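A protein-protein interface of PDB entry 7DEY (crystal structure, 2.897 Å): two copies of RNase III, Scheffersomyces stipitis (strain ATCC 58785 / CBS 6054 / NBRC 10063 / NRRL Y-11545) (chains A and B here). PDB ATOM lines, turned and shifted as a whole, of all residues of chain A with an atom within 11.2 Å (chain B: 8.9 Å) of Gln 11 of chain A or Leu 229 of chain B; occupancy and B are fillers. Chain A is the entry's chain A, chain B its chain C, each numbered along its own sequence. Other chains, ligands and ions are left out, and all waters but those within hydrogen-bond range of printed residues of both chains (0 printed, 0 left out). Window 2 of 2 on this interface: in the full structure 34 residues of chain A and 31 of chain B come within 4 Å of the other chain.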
ATOM      1  N   PHE A   7       2.904  13.448 -21.070  1.00  0.00           N
ATOM      2  CA  PHE A   7       1.906  12.668 -20.374  1.00  0.00           C
ATOM      3  C   PHE A   7       1.747  13.159 -18.936  1.00  0.00           C
ATOM      4  O   PHE A   7       2.697  13.628 -18.305  1.00  0.00           O
ATOM      5  CB  PHE A   7       2.324  11.201 -20.410  1.00  0.00           C
ATOM      6  CG  PHE A   7       1.352  10.276 -19.765  1.00  0.00           C
ATOM      7  CD1 PHE A   7       0.055  10.202 -20.219  1.00  0.00           C
ATOM      8  CD2 PHE A   7       1.742   9.480 -18.710  1.00  0.00           C
ATOM      9  CE1 PHE A   7      -0.829   9.382 -19.629  1.00  0.00           C
ATOM     10  CE2 PHE A   7       0.870   8.637 -18.113  1.00  0.00           C
ATOM     11  CZ  PHE A   7      -0.426   8.586 -18.564  1.00  0.00           C
ATOM     12  N   ILE A   8       0.524  13.065 -18.430  1.00  0.00           N
ATOM     13  CA  ILE A   8       0.228  13.328 -17.031  1.00  0.00           C
ATOM     14  C   ILE A   8      -0.080  11.991 -16.378  1.00  0.00           C
ATOM     15  O   ILE A   8      -1.086  11.342 -16.711  1.00  0.00           O
ATOM     16  CB  ILE A   8      -0.949  14.302 -16.863  1.00  0.00           C
ATOM     17  CG1 ILE A   8      -0.560  15.715 -17.300  1.00  0.00           C
ATOM     18  CG2 ILE A   8      -1.443  14.300 -15.402  1.00  0.00           C
ATOM     19  CD1 ILE A   8      -1.659  16.708 -17.106  1.00  0.00           C
ATOM     20  N   LYS A   9       0.772  11.587 -15.438  1.00  0.00           N
ATOM     21  CA  LYS A   9       0.594  10.287 -14.812  1.00  0.00           C
ATOM     22  C   LYS A   9      -0.484  10.325 -13.730  1.00  0.00           C
ATOM     23  O   LYS A   9      -1.351   9.445 -13.690  1.00  0.00           O
ATOM     24  CB  LYS A   9       1.935   9.809 -14.265  1.00  0.00           C
ATOM     25  CG  LYS A   9       1.970   8.373 -13.858  1.00  0.00           C
ATOM     26  CD  LYS A   9       3.355   7.994 -13.343  1.00  0.00           C
ATOM     27  CE  LYS A   9       4.008   6.921 -14.225  1.00  0.00           C
ATOM     28  NZ  LYS A   9       5.516   6.892 -14.155  1.00  0.00           N
ATOM     29  N   ASP A  10      -0.492  11.352 -12.884  1.00  0.00           N
ATOM     30  CA  ASP A  10      -1.415  11.382 -11.747  1.00  0.00           C
ATOM     31  C   ASP A  10      -2.854  11.650 -12.186  1.00  0.00           C
ATOM     32  O   ASP A  10      -3.161  12.742 -12.674  1.00  0.00           O
ATOM     33  CB  ASP A  10      -0.980  12.450 -10.753  1.00  0.00           C
ATOM     34  CG  ASP A  10      -1.829  12.452  -9.499  1.00  0.00           C
ATOM     35  OD1 ASP A  10      -2.678  11.547  -9.319  1.00  0.00           O
ATOM     36  OD2 ASP A  10      -1.633  13.352  -8.664  1.00  0.00           O
ATOM     37  N   GLN A  11      -3.756  10.694 -11.947  1.00  0.00           N
ATOM     38  CA  GLN A  11      -5.138  10.863 -12.399  1.00  0.00           C
ATOM     39  C   GLN A  11      -5.761  12.145 -11.847  1.00  0.00           C
ATOM     40  O   GLN A  11      -6.229  12.994 -12.605  1.00  0.00           O
ATOM     41  CB  GLN A  11      -5.975   9.652 -12.012  1.00  0.00           C
ATOM     42  CG  GLN A  11      -6.021   8.579 -13.060  1.00  0.00           C
ATOM     43  CD  GLN A  11      -6.636   9.039 -14.352  1.00  0.00           C
ATOM     44  OE1 GLN A  11      -5.967   9.636 -15.183  1.00  0.00           O
ATOM     45  NE2 GLN A  11      -7.917   8.761 -14.534  1.00  0.00           N
ATOM     46  N   THR A  12      -5.755  12.319 -10.529  1.00  0.00           N
ATOM     47  CA  THR A  12      -6.455  13.462  -9.958  1.00  0.00           C
ATOM     48  C   THR A  12      -5.848  14.787 -10.419  1.00  0.00           C
ATOM     49  O   THR A  12      -6.568  15.777 -10.591  1.00  0.00           O
ATOM     50  CB  THR A  12      -6.461  13.371  -8.432  1.00  0.00           C
ATOM     51  OG1 THR A  12      -5.221  13.862  -7.939  1.00  0.00           O
ATOM     52  CG2 THR A  12      -6.666  11.926  -7.961  1.00  0.00           C
ATOM     53  N   LEU A  13      -4.538  14.821 -10.664  1.00  0.00           N
ATOM     54  CA  LEU A  13      -3.931  16.045 -11.187  1.00  0.00           C
ATOM     55  C   LEU A  13      -4.352  16.275 -12.641  1.00  0.00           C
ATOM     56  O   LEU A  13      -4.554  17.419 -13.063  1.00  0.00           O
ATOM     57  CB  LEU A  13      -2.400  15.987 -11.001  1.00  0.00           C
ATOM     58  CG  LEU A  13      -1.469  17.030 -11.615  1.00  0.00           C
ATOM     59  CD1 LEU A  13      -1.789  18.335 -10.950  1.00  0.00           C
ATOM     60  CD2 LEU A  13       0.027  16.719 -11.387  1.00  0.00           C
ATOM     61  N   TYR A  14      -4.538  15.193 -13.404  1.00  0.00           N
ATOM     62  CA  TYR A  14      -5.128  15.301 -14.735  1.00  0.00           C
ATOM     63  C   TYR A  14      -6.532  15.877 -14.676  1.00  0.00           C
ATOM     64  O   TYR A  14      -6.919  16.685 -15.530  1.00  0.00           O
ATOM     65  CB  TYR A  14      -5.173  13.929 -15.396  1.00  0.00           C
ATOM     66  CG  TYR A  14      -5.845  13.924 -16.743  1.00  0.00           C
ATOM     67  CD1 TYR A  14      -5.136  14.284 -17.887  1.00  0.00           C
ATOM     68  CD2 TYR A  14      -7.174  13.547 -16.886  1.00  0.00           C
ATOM     69  CE1 TYR A  14      -5.726  14.276 -19.141  1.00  0.00           C
ATOM     70  CE2 TYR A  14      -7.778  13.540 -18.147  1.00  0.00           C
ATOM     71  CZ  TYR A  14      -7.042  13.908 -19.267  1.00  0.00           C
ATOM     72  OH  TYR A  14      -7.605  13.901 -20.519  1.00  0.00           O
ATOM     73  N   GLU A  15      -7.328  15.430 -13.703  1.00  0.00           N
ATOM     74  CA  GLU A  15      -8.705  15.888 -13.594  1.00  0.00           C
ATOM     75  C   GLU A  15      -8.763  17.338 -13.142  1.00  0.00           C
ATOM     76  O   GLU A  15      -9.724  18.040 -13.456  1.00  0.00           O
ATOM     77  CB  GLU A  15      -9.468  14.951 -12.643  1.00  0.00           C
ATOM     78  CG  GLU A  15      -9.219  13.444 -12.951  1.00  0.00           C
ATOM     79  CD  GLU A  15     -10.201  12.471 -12.304  1.00  0.00           C
ATOM     80  OE1 GLU A  15     -10.467  11.408 -12.906  1.00  0.00           O
ATOM     81  OE2 GLU A  15     -10.687  12.755 -11.188  1.00  0.00           O
ATOM     82  N   ARG A  16      -7.731  17.808 -12.454  1.00  0.00           N
ATOM     83  CA  ARG A  16      -7.653  19.183 -11.996  1.00  0.00           C
ATOM     84  C   ARG A  16      -7.283  20.141 -13.131  1.00  0.00           C
ATOM     85  O   ARG A  16      -7.122  21.341 -12.901  1.00  0.00           O
ATOM     86  CB  ARG A  16      -6.680  19.255 -10.785  1.00  0.00           C
ATOM     87  CG  ARG A  16      -6.726  20.526  -9.945  1.00  0.00           C
ATOM     88  CD  ARG A  16      -6.262  20.365  -8.509  1.00  0.00           C
ATOM     89  NE  ARG A  16      -7.334  20.646  -7.538  1.00  0.00           N
ATOM     90  CZ  ARG A  16      -7.954  21.819  -7.374  1.00  0.00           C
ATOM     91  NH1 ARG A  16      -7.638  22.875  -8.129  1.00  0.00           N
ATOM     92  NH2 ARG A  16      -8.905  21.934  -6.445  1.00  0.00           N
ATOM     93  N   VAL A  17      -7.181  19.659 -14.366  1.00  0.00           N
ATOM     94  CA  VAL A  17      -7.055  20.551 -15.512  1.00  0.00           C
ATOM     95  C   VAL A  17      -8.139  20.329 -16.563  1.00  0.00           C
ATOM     96  O   VAL A  17      -8.492  21.284 -17.275  1.00  0.00           O
ATOM     97  CB  VAL A  17      -5.648  20.439 -16.144  1.00  0.00           C
ATOM     98  CG1 VAL A  17      -5.258  19.005 -16.332  1.00  0.00           C
ATOM     99  CG2 VAL A  17      -5.528  21.213 -17.463  1.00  0.00           C
ATOM    100  N   PHE A  18      -8.755  19.144 -16.626  1.00  0.00           N
ATOM    101  CA  PHE A  18      -9.653  18.768 -17.713  1.00  0.00           C
ATOM    102  C   PHE A  18     -11.101  18.512 -17.310  1.00  0.00           C
ATOM    103  O   PHE A  18     -12.001  18.864 -18.070  1.00  0.00           O
ATOM    104  CB  PHE A  18      -9.098  17.529 -18.412  1.00  0.00           C
ATOM    105  CG  PHE A  18      -7.948  17.827 -19.312  1.00  0.00           C
ATOM    106  CD1 PHE A  18      -8.140  18.540 -20.477  1.00  0.00           C
ATOM    107  CD2 PHE A  18      -6.676  17.421 -18.979  1.00  0.00           C
ATOM    108  CE1 PHE A  18      -7.090  18.825 -21.304  1.00  0.00           C
ATOM    109  CE2 PHE A  18      -5.609  17.708 -19.795  1.00  0.00           C
ATOM    110  CZ  PHE A  18      -5.816  18.414 -20.963  1.00  0.00           C
ATOM    111  N   VAL A  19     -11.379  17.882 -16.164  1.00  0.00           N
ATOM    112  CA  VAL A  19     -12.780  17.652 -15.808  1.00  0.00           C
ATOM    113  C   VAL A  19     -13.389  18.851 -15.082  1.00  0.00           C
ATOM    114  O   VAL A  19     -14.625  18.961 -15.012  1.00  0.00           O
ATOM    115  CB  VAL A  19     -12.979  16.373 -14.963  1.00  0.00           C
ATOM    116  CG1 VAL A  19     -12.167  15.193 -15.528  1.00  0.00           C
ATOM    117  CG2 VAL A  19     -12.683  16.618 -13.473  1.00  0.00           C
ATOM    118  N   HIS A  20     -12.561  19.750 -14.553  1.00  0.00           N
ATOM    119  CA  HIS A  20     -13.029  20.974 -13.912  1.00  0.00           C
ATOM    120  C   HIS A  20     -12.802  22.166 -14.845  1.00  0.00           C
ATOM    121  O   HIS A  20     -12.273  22.009 -15.954  1.00  0.00           O
ATOM    122  CB  HIS A  20     -12.320  21.186 -12.576  1.00  0.00           C
ATOM    123  N   ASN A  40      -9.524  24.125 -11.498  1.00  0.00           N
ATOM    124  CA  ASN A  40      -8.210  24.148 -12.133  1.00  0.00           C
ATOM    125  C   ASN A  40      -7.336  25.278 -11.584  1.00  0.00           C
ATOM    126  O   ASN A  40      -6.160  25.416 -11.971  1.00  0.00           O
ATOM    127  CB  ASN A  40      -8.353  24.285 -13.650  1.00  0.00           C
ATOM    128  CG  ASN A  40      -9.260  23.218 -14.251  1.00  0.00           C
ATOM    129  OD1 ASN A  40      -9.527  22.183 -13.625  1.00  0.00           O
ATOM    130  ND2 ASN A  40      -9.734  23.460 -15.483  1.00  0.00           N
ATOM    131  N   LEU A  43      -3.199  26.244 -10.863  1.00  0.00           N
ATOM    132  CA  LEU A  43      -2.326  25.572 -11.814  1.00  0.00           C
ATOM    133  C   LEU A  43      -2.135  26.405 -13.071  1.00  0.00           C
ATOM    134  O   LEU A  43      -1.093  26.306 -13.727  1.00  0.00           O
ATOM    135  CB  LEU A  43      -2.903  24.216 -12.204  1.00  0.00           C
ATOM    136  CG  LEU A  43      -2.807  23.013 -11.281  1.00  0.00           C
ATOM    137  CD1 LEU A  43      -3.459  21.831 -11.984  1.00  0.00           C
ATOM    138  CD2 LEU A  43      -1.367  22.716 -10.923  1.00  0.00           C
ATOM    139  N   ARG A  96     -10.286  16.050 -24.852  1.00  0.00           N
ATOM    140  CA  ARG A  96     -10.071  15.647 -23.464  1.00  0.00           C
ATOM    141  C   ARG A  96     -11.018  16.392 -22.527  1.00  0.00           C
ATOM    142  O   ARG A  96     -11.404  15.867 -21.481  1.00  0.00           O
ATOM    143  CB  ARG A  96      -8.607  15.878 -23.075  1.00  0.00           C
ATOM    144  CG  ARG A  96      -7.636  15.480 -24.179  1.00  0.00           C
ATOM    145  CD  ARG A  96      -6.187  15.473 -23.720  1.00  0.00           C
ATOM    146  NE  ARG A  96      -5.248  15.360 -24.838  1.00  0.00           N
ATOM    147  CZ  ARG A  96      -4.847  14.206 -25.368  1.00  0.00           C
ATOM    148  NH1 ARG A  96      -5.305  13.057 -24.889  1.00  0.00           N
ATOM    149  NH2 ARG A  96      -3.989  14.194 -26.381  1.00  0.00           N
ATOM    150  N   LYS A  98     -14.372  17.694 -20.979  1.00  0.00           N
ATOM    151  CA  LYS A  98     -15.756  17.236 -20.845  1.00  0.00           C
ATOM    152  C   LYS A  98     -16.689  18.426 -20.629  1.00  0.00           C
ATOM    153  O   LYS A  98     -16.327  19.404 -19.963  1.00  0.00           O
ATOM    154  CB  LYS A  98     -15.898  16.233 -19.686  1.00  0.00           C
ATOM    155  CG  LYS A  98     -14.957  15.033 -19.746  1.00  0.00           C
ATOM    156  CD  LYS A  98     -15.039  14.323 -21.091  1.00  0.00           C
ATOM    157  CE  LYS A  98     -13.735  13.602 -21.398  1.00  0.00           C
ATOM    158  NZ  LYS A  98     -13.545  13.439 -22.870  1.00  0.00           N
ATOM    159  N   TYR A 121      -2.188  23.191 -17.963  1.00  0.00           N
ATOM    160  CA  TYR A 121      -1.503  21.971 -18.373  1.00  0.00           C
ATOM    161  C   TYR A 121      -0.004  22.077 -18.138  1.00  0.00           C
ATOM    162  O   TYR A 121       0.595  21.189 -17.523  1.00  0.00           O
ATOM    163  CB  TYR A 121      -1.783  21.663 -19.843  1.00  0.00           C
ATOM    164  CG  TYR A 121      -1.376  20.249 -20.227  1.00  0.00           C
ATOM    165  CD1 TYR A 121      -0.086  19.963 -20.670  1.00  0.00           C
ATOM    166  CD2 TYR A 121      -2.283  19.199 -20.122  1.00  0.00           C
ATOM    167  CE1 TYR A 121       0.275  18.670 -21.005  1.00  0.00           C
ATOM    168  CE2 TYR A 121      -1.935  17.919 -20.456  1.00  0.00           C
ATOM    169  CZ  TYR A 121      -0.660  17.654 -20.893  1.00  0.00           C
ATOM    170  OH  TYR A 121      -0.339  16.357 -21.219  1.00  0.00           O
ATOM    171  N   ALA A 124       0.550  21.592 -14.514  1.00  0.00           N
ATOM    172  CA  ALA A 124       0.520  20.167 -14.202  1.00  0.00           C
ATOM    173  C   ALA A 124       1.848  19.498 -14.542  1.00  0.00           C
ATOM    174  O   ALA A 124       2.481  18.880 -13.675  1.00  0.00           O
ATOM    175  CB  ALA A 124      -0.623  19.493 -14.956  1.00  0.00           C
ATOM    176  N   GLU A 128       4.172  17.787 -11.348  1.00  0.00           N
ATOM    177  CA  GLU A 128       4.537  16.383 -11.493  1.00  0.00           C
ATOM    178  C   GLU A 128       6.034  16.153 -11.670  1.00  0.00           C
ATOM    179  O   GLU A 128       6.485  15.007 -11.560  1.00  0.00           O
ATOM    180  CB  GLU A 128       3.798  15.767 -12.689  1.00  0.00           C
ATOM    181  CG  GLU A 128       3.557  14.306 -12.492  1.00  0.00           C
ATOM    182  CD  GLU A 128       2.961  13.629 -13.689  1.00  0.00           C
ATOM    183  OE1 GLU A 128       1.739  13.330 -13.622  1.00  0.00           O
ATOM    184  OE2 GLU A 128       3.711  13.378 -14.674  1.00  0.00           O
ATOM    185  N   GLU B 167       1.148   4.369 -21.438  1.00  0.00           N
ATOM    186  CA  GLU B 167       0.445   5.426 -20.706  1.00  0.00           C
ATOM    187  C   GLU B 167      -0.960   4.971 -20.336  1.00  0.00           C
ATOM    188  O   GLU B 167      -1.384   5.103 -19.179  1.00  0.00           O
ATOM    189  CB  GLU B 167       0.405   6.725 -21.527  1.00  0.00           C
ATOM    190  N   LEU B 168      -1.677   4.383 -21.312  1.00  0.00           N
ATOM    191  CA  LEU B 168      -3.011   3.836 -21.057  1.00  0.00           C
ATOM    192  C   LEU B 168      -2.951   2.636 -20.112  1.00  0.00           C
ATOM    193  O   LEU B 168      -3.845   2.458 -19.274  1.00  0.00           O
ATOM    194  CB  LEU B 168      -3.681   3.455 -22.381  1.00  0.00           C
ATOM    195  CG  LEU B 168      -4.770   2.375 -22.311  1.00  0.00           C
ATOM    196  CD1 LEU B 168      -5.992   2.818 -21.486  1.00  0.00           C
ATOM    197  CD2 LEU B 168      -5.191   1.965 -23.701  1.00  0.00           C
ATOM    198  N   SER B 170      -0.755   2.185 -17.671  1.00  0.00           N
ATOM    199  CA  SER B 170      -0.523   2.695 -16.321  1.00  0.00           C
ATOM    200  C   SER B 170      -1.769   3.318 -15.690  1.00  0.00           C
ATOM    201  O   SER B 170      -1.712   3.761 -14.535  1.00  0.00           O
ATOM    202  CB  SER B 170       0.621   3.715 -16.331  1.00  0.00           C
ATOM    203  OG  SER B 170       0.150   5.014 -16.639  1.00  0.00           O
ATOM    204  N   ILE B 171      -2.888   3.376 -16.398  1.00  0.00           N
ATOM    205  CA  ILE B 171      -4.107   3.849 -15.765  1.00  0.00           C
ATOM    206  C   ILE B 171      -4.968   2.650 -15.402  1.00  0.00           C
ATOM    207  O   ILE B 171      -5.592   2.617 -14.335  1.00  0.00           O
ATOM    208  CB  ILE B 171      -4.851   4.839 -16.676  1.00  0.00           C
ATOM    209  CG1 ILE B 171      -3.939   6.018 -16.981  1.00  0.00           C
ATOM    210  CG2 ILE B 171      -6.159   5.296 -16.036  1.00  0.00           C
ATOM    211  CD1 ILE B 171      -4.488   6.974 -17.959  1.00  0.00           C
ATOM    212  N   VAL B 172      -4.982   1.643 -16.272  1.00  0.00           N
ATOM    213  CA  VAL B 172      -5.994   0.599 -16.175  1.00  0.00           C
ATOM    214  C   VAL B 172      -5.410  -0.811 -16.270  1.00  0.00           C
ATOM    215  O   VAL B 172      -6.155  -1.796 -16.297  1.00  0.00           O
ATOM    216  CB  VAL B 172      -7.069   0.848 -17.251  1.00  0.00           C
ATOM    217  CG1 VAL B 172      -6.558   0.447 -18.616  1.00  0.00           C
ATOM    218  CG2 VAL B 172      -8.389   0.151 -16.892  1.00  0.00           C
ATOM    219  N   MET B 199     -10.475  -3.976 -23.248  1.00  0.00           N
ATOM    220  CA  MET B 199     -10.097  -4.414 -21.911  1.00  0.00           C
ATOM    221  C   MET B 199     -11.123  -5.467 -21.484  1.00  0.00           C
ATOM    222  O   MET B 199     -12.077  -5.193 -20.756  1.00  0.00           O
ATOM    223  CB  MET B 199     -10.026  -3.167 -20.946  1.00  0.00           C
ATOM    224  CG  MET B 199     -10.071  -3.423 -19.435  1.00  0.00           C
ATOM    225  SD  MET B 199      -8.513  -3.977 -18.718  1.00  0.00           S
ATOM    226  CE  MET B 199      -7.401  -2.878 -19.564  1.00  0.00           C
ATOM    227  N   LEU B 224      -7.606   7.304 -24.017  1.00  0.00           N
ATOM    228  CA  LEU B 224      -7.153   8.281 -23.027  1.00  0.00           C
ATOM    229  C   LEU B 224      -7.866   9.622 -23.112  1.00  0.00           C
ATOM    230  O   LEU B 224      -7.860  10.382 -22.133  1.00  0.00           O
ATOM    231  CB  LEU B 224      -5.647   8.516 -23.178  1.00  0.00           C
ATOM    232  CG  LEU B 224      -4.849   7.242 -22.968  1.00  0.00           C
ATOM    233  CD1 LEU B 224      -3.557   7.274 -23.743  1.00  0.00           C
ATOM    234  CD2 LEU B 224      -4.619   7.062 -21.470  1.00  0.00           C
ATOM    235  N   ASN B 226     -10.695   9.895 -22.737  1.00  0.00           N
ATOM    236  CA  ASN B 226     -11.788   9.724 -21.783  1.00  0.00           C
ATOM    237  C   ASN B 226     -11.263   9.027 -20.535  1.00  0.00           C
ATOM    238  O   ASN B 226     -11.398   7.811 -20.394  1.00  0.00           O
ATOM    239  CB  ASN B 226     -12.932   8.949 -22.409  1.00  0.00           C
ATOM    240  CG  ASN B 226     -13.938   9.852 -23.033  1.00  0.00           C
ATOM    241  OD1 ASN B 226     -14.544  10.674 -22.353  1.00  0.00           O
ATOM    242  ND2 ASN B 226     -14.111   9.734 -24.340  1.00  0.00           N
ATOM    243  N   ARG B 227     -10.702   9.797 -19.614  1.00  0.00           N
ATOM    244  CA  ARG B 227     -10.189   9.258 -18.363  1.00  0.00           C
ATOM    245  C   ARG B 227     -11.266   9.404 -17.290  1.00  0.00           C
ATOM    246  O   ARG B 227     -11.685  10.521 -16.959  1.00  0.00           O
ATOM    247  CB  ARG B 227      -8.897   9.960 -17.950  1.00  0.00           C
ATOM    248  CG  ARG B 227      -7.680   9.539 -18.746  1.00  0.00           C
ATOM    249  CD  ARG B 227      -6.396   9.938 -18.018  1.00  0.00           C
ATOM    250  NE  ARG B 227      -5.381  10.531 -18.883  1.00  0.00           N
ATOM    251  CZ  ARG B 227      -4.196  10.973 -18.462  1.00  0.00           C
ATOM    252  NH1 ARG B 227      -3.866  10.884 -17.179  1.00  0.00           N
ATOM    253  NH2 ARG B 227      -3.336  11.504 -19.333  1.00  0.00           N
ATOM    254  N   GLN B 228     -11.731   8.267 -16.777  1.00  0.00           N
ATOM    255  CA  GLN B 228     -12.858   8.233 -15.856  1.00  0.00           C
ATOM    256  C   GLN B 228     -12.511   7.631 -14.499  1.00  0.00           C
ATOM    257  O   GLN B 228     -12.693   8.298 -13.475  1.00  0.00           O
ATOM    258  CB  GLN B 228     -14.001   7.462 -16.531  1.00  0.00           C
ATOM    259  CG  GLN B 228     -13.511   6.344 -17.454  1.00  0.00           C
ATOM    260  CD  GLN B 228     -12.979   5.140 -16.688  1.00  0.00           C
ATOM    261  OE1 GLN B 228     -13.715   4.510 -15.914  1.00  0.00           O
ATOM    262  NE2 GLN B 228     -11.694   4.825 -16.881  1.00  0.00           N
ATOM    263  N   LEU B 229     -11.987   6.404 -14.450  1.00  0.00           N
ATOM    264  CA  LEU B 229     -12.013   5.641 -13.203  1.00  0.00           C
ATOM    265  C   LEU B 229     -11.034   6.249 -12.208  1.00  0.00           C
ATOM    266  O   LEU B 229      -9.810   6.145 -12.364  1.00  0.00           O
ATOM    267  CB  LEU B 229     -11.737   4.160 -13.449  1.00  0.00           C
ATOM    268  CG  LEU B 229     -12.708   3.261 -12.657  1.00  0.00           C
ATOM    269  CD1 LEU B 229     -14.177   3.463 -13.080  1.00  0.00           C
ATOM    270  CD2 LEU B 229     -12.321   1.771 -12.704  1.00  0.00           C
ATOM    271  N   LEU B 230     -11.595   6.851 -11.165  1.00  0.00           N
ATOM    272  CA  LEU B 230     -10.899   7.792 -10.305  1.00  0.00           C
ATOM    273  C   LEU B 230      -9.839   7.130  -9.420  1.00  0.00           C
ATOM    274  O   LEU B 230      -8.643   7.403  -9.567  1.00  0.00           O
ATOM    275  CB  LEU B 230     -11.943   8.531  -9.460  1.00  0.00           C
ATOM    276  CG  LEU B 230     -13.081   9.090 -10.337  1.00  0.00           C
ATOM    277  CD1 LEU B 230     -14.256   8.120 -10.449  1.00  0.00           C
ATOM    278  CD2 LEU B 230     -13.547  10.439  -9.824  1.00  0.00           C
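Of the 12 printed residues of chain B, 8 touch a printed residue of chain A.
Printed residues of chain B that touch a printed residue of chain A: Glu 167, Ser 170, Leu 224, Asn 226, Arg 227, Gln 228, Leu 229 and Leu 230.
Hydrophobic or aromatic side chains of chain A within 4 Å of the printed part of chain B: Phe 7 and Tyr 14.
Among the printed residues, 11 pairs touch across the chains.
Gln 11 of chain A touches two residues of chain B.
Leu 229 of chain B touches just one residue of chain A: Gln 11.
Asp 10 of chain A touches none of the printed residues of chain B.
No residue of chain B comes within 4 Å of Thr 12 of chain A.
Gln 228 of chain B touches just one residue of chain A: Glu 15.
Of chain A, only Glu 15 (3.9 Å) comes within 4 Å of Leu 230 of chain B.
Printed residues of chain B within 4 Å of Lys 98 of chain A: Asn 226.
Of the printed residues of chain B, Ile 8 of chain A touches Arg 227.
Of the printed residues of chain A, Leu 224 of chain B touches Tyr 14.
Val 172 of chain B touches none of the printed residues of chain A.
The nearest residue of chain B that does not touch Gln 11 of chain A is Ile 171 of chain B (4.1 Å).
The nearest residue of chain A that does not touch Leu 229 of chain B is Glu 15 of chain A (5.2 Å).
The backbone carbonyl oxygen (O) of Ile 8 of chain A is in hydrogen-bond range of the guanidinium group (NH1) of Arg 227 of chain B (2.9 Å).
The guanidinium group (NH1) of Arg 227 of chain B lies close to the side-chain amide oxygen (OE1) of Gln 11 of chain A (3.2 Å).
The side-chain amide oxygen (OD1) of Asn 226 of chain B sits at hydrogen-bond distance from the side-chain amino group (NZ) of Lys 98 of chain A (3.0 Å).
No position is printed for both chains.
Of the 11 pairs that touch across the chains among the printed residues, none has its exchanged pair printed and touching as well.
The backbone carbonyl oxygen of Glu 15 of chain A lies within hydrogen-bond range of the backbone NH of His 20 of chain A, 3.5 Å away.
OG of Ser 170 of chain B lies within hydrogen-bond range of O of Glu 167 of chain B (3.0 Å).
Phe 7 of chain A touches Glu 167 of chain B (CE1 to CB, 3.5 Å).
Ser 170 of chain B touches Phe 7 of chain A (OG to CE2, 3.98 Å).
NH2 of Arg 227 of chain B touches CE1 of Phe 7 of chain A, at 3.3 Å.
NE2 of Gln 11 of chain A touches O of Leu 229 of chain B, at 3.9 Å.
Leu 224 of chain B touches Tyr 14 of chain A (O to OH, 3.9 Å).
Tyr 14 of chain A touches Arg 227 of chain B (CD1 to CZ, 3.5 Å).
Gln 228 of chain B touches Glu 15 of chain A.
OE2 of Glu 15 of chain A touches CD2 of Leu 230 of chain B, at 3.9 Å.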
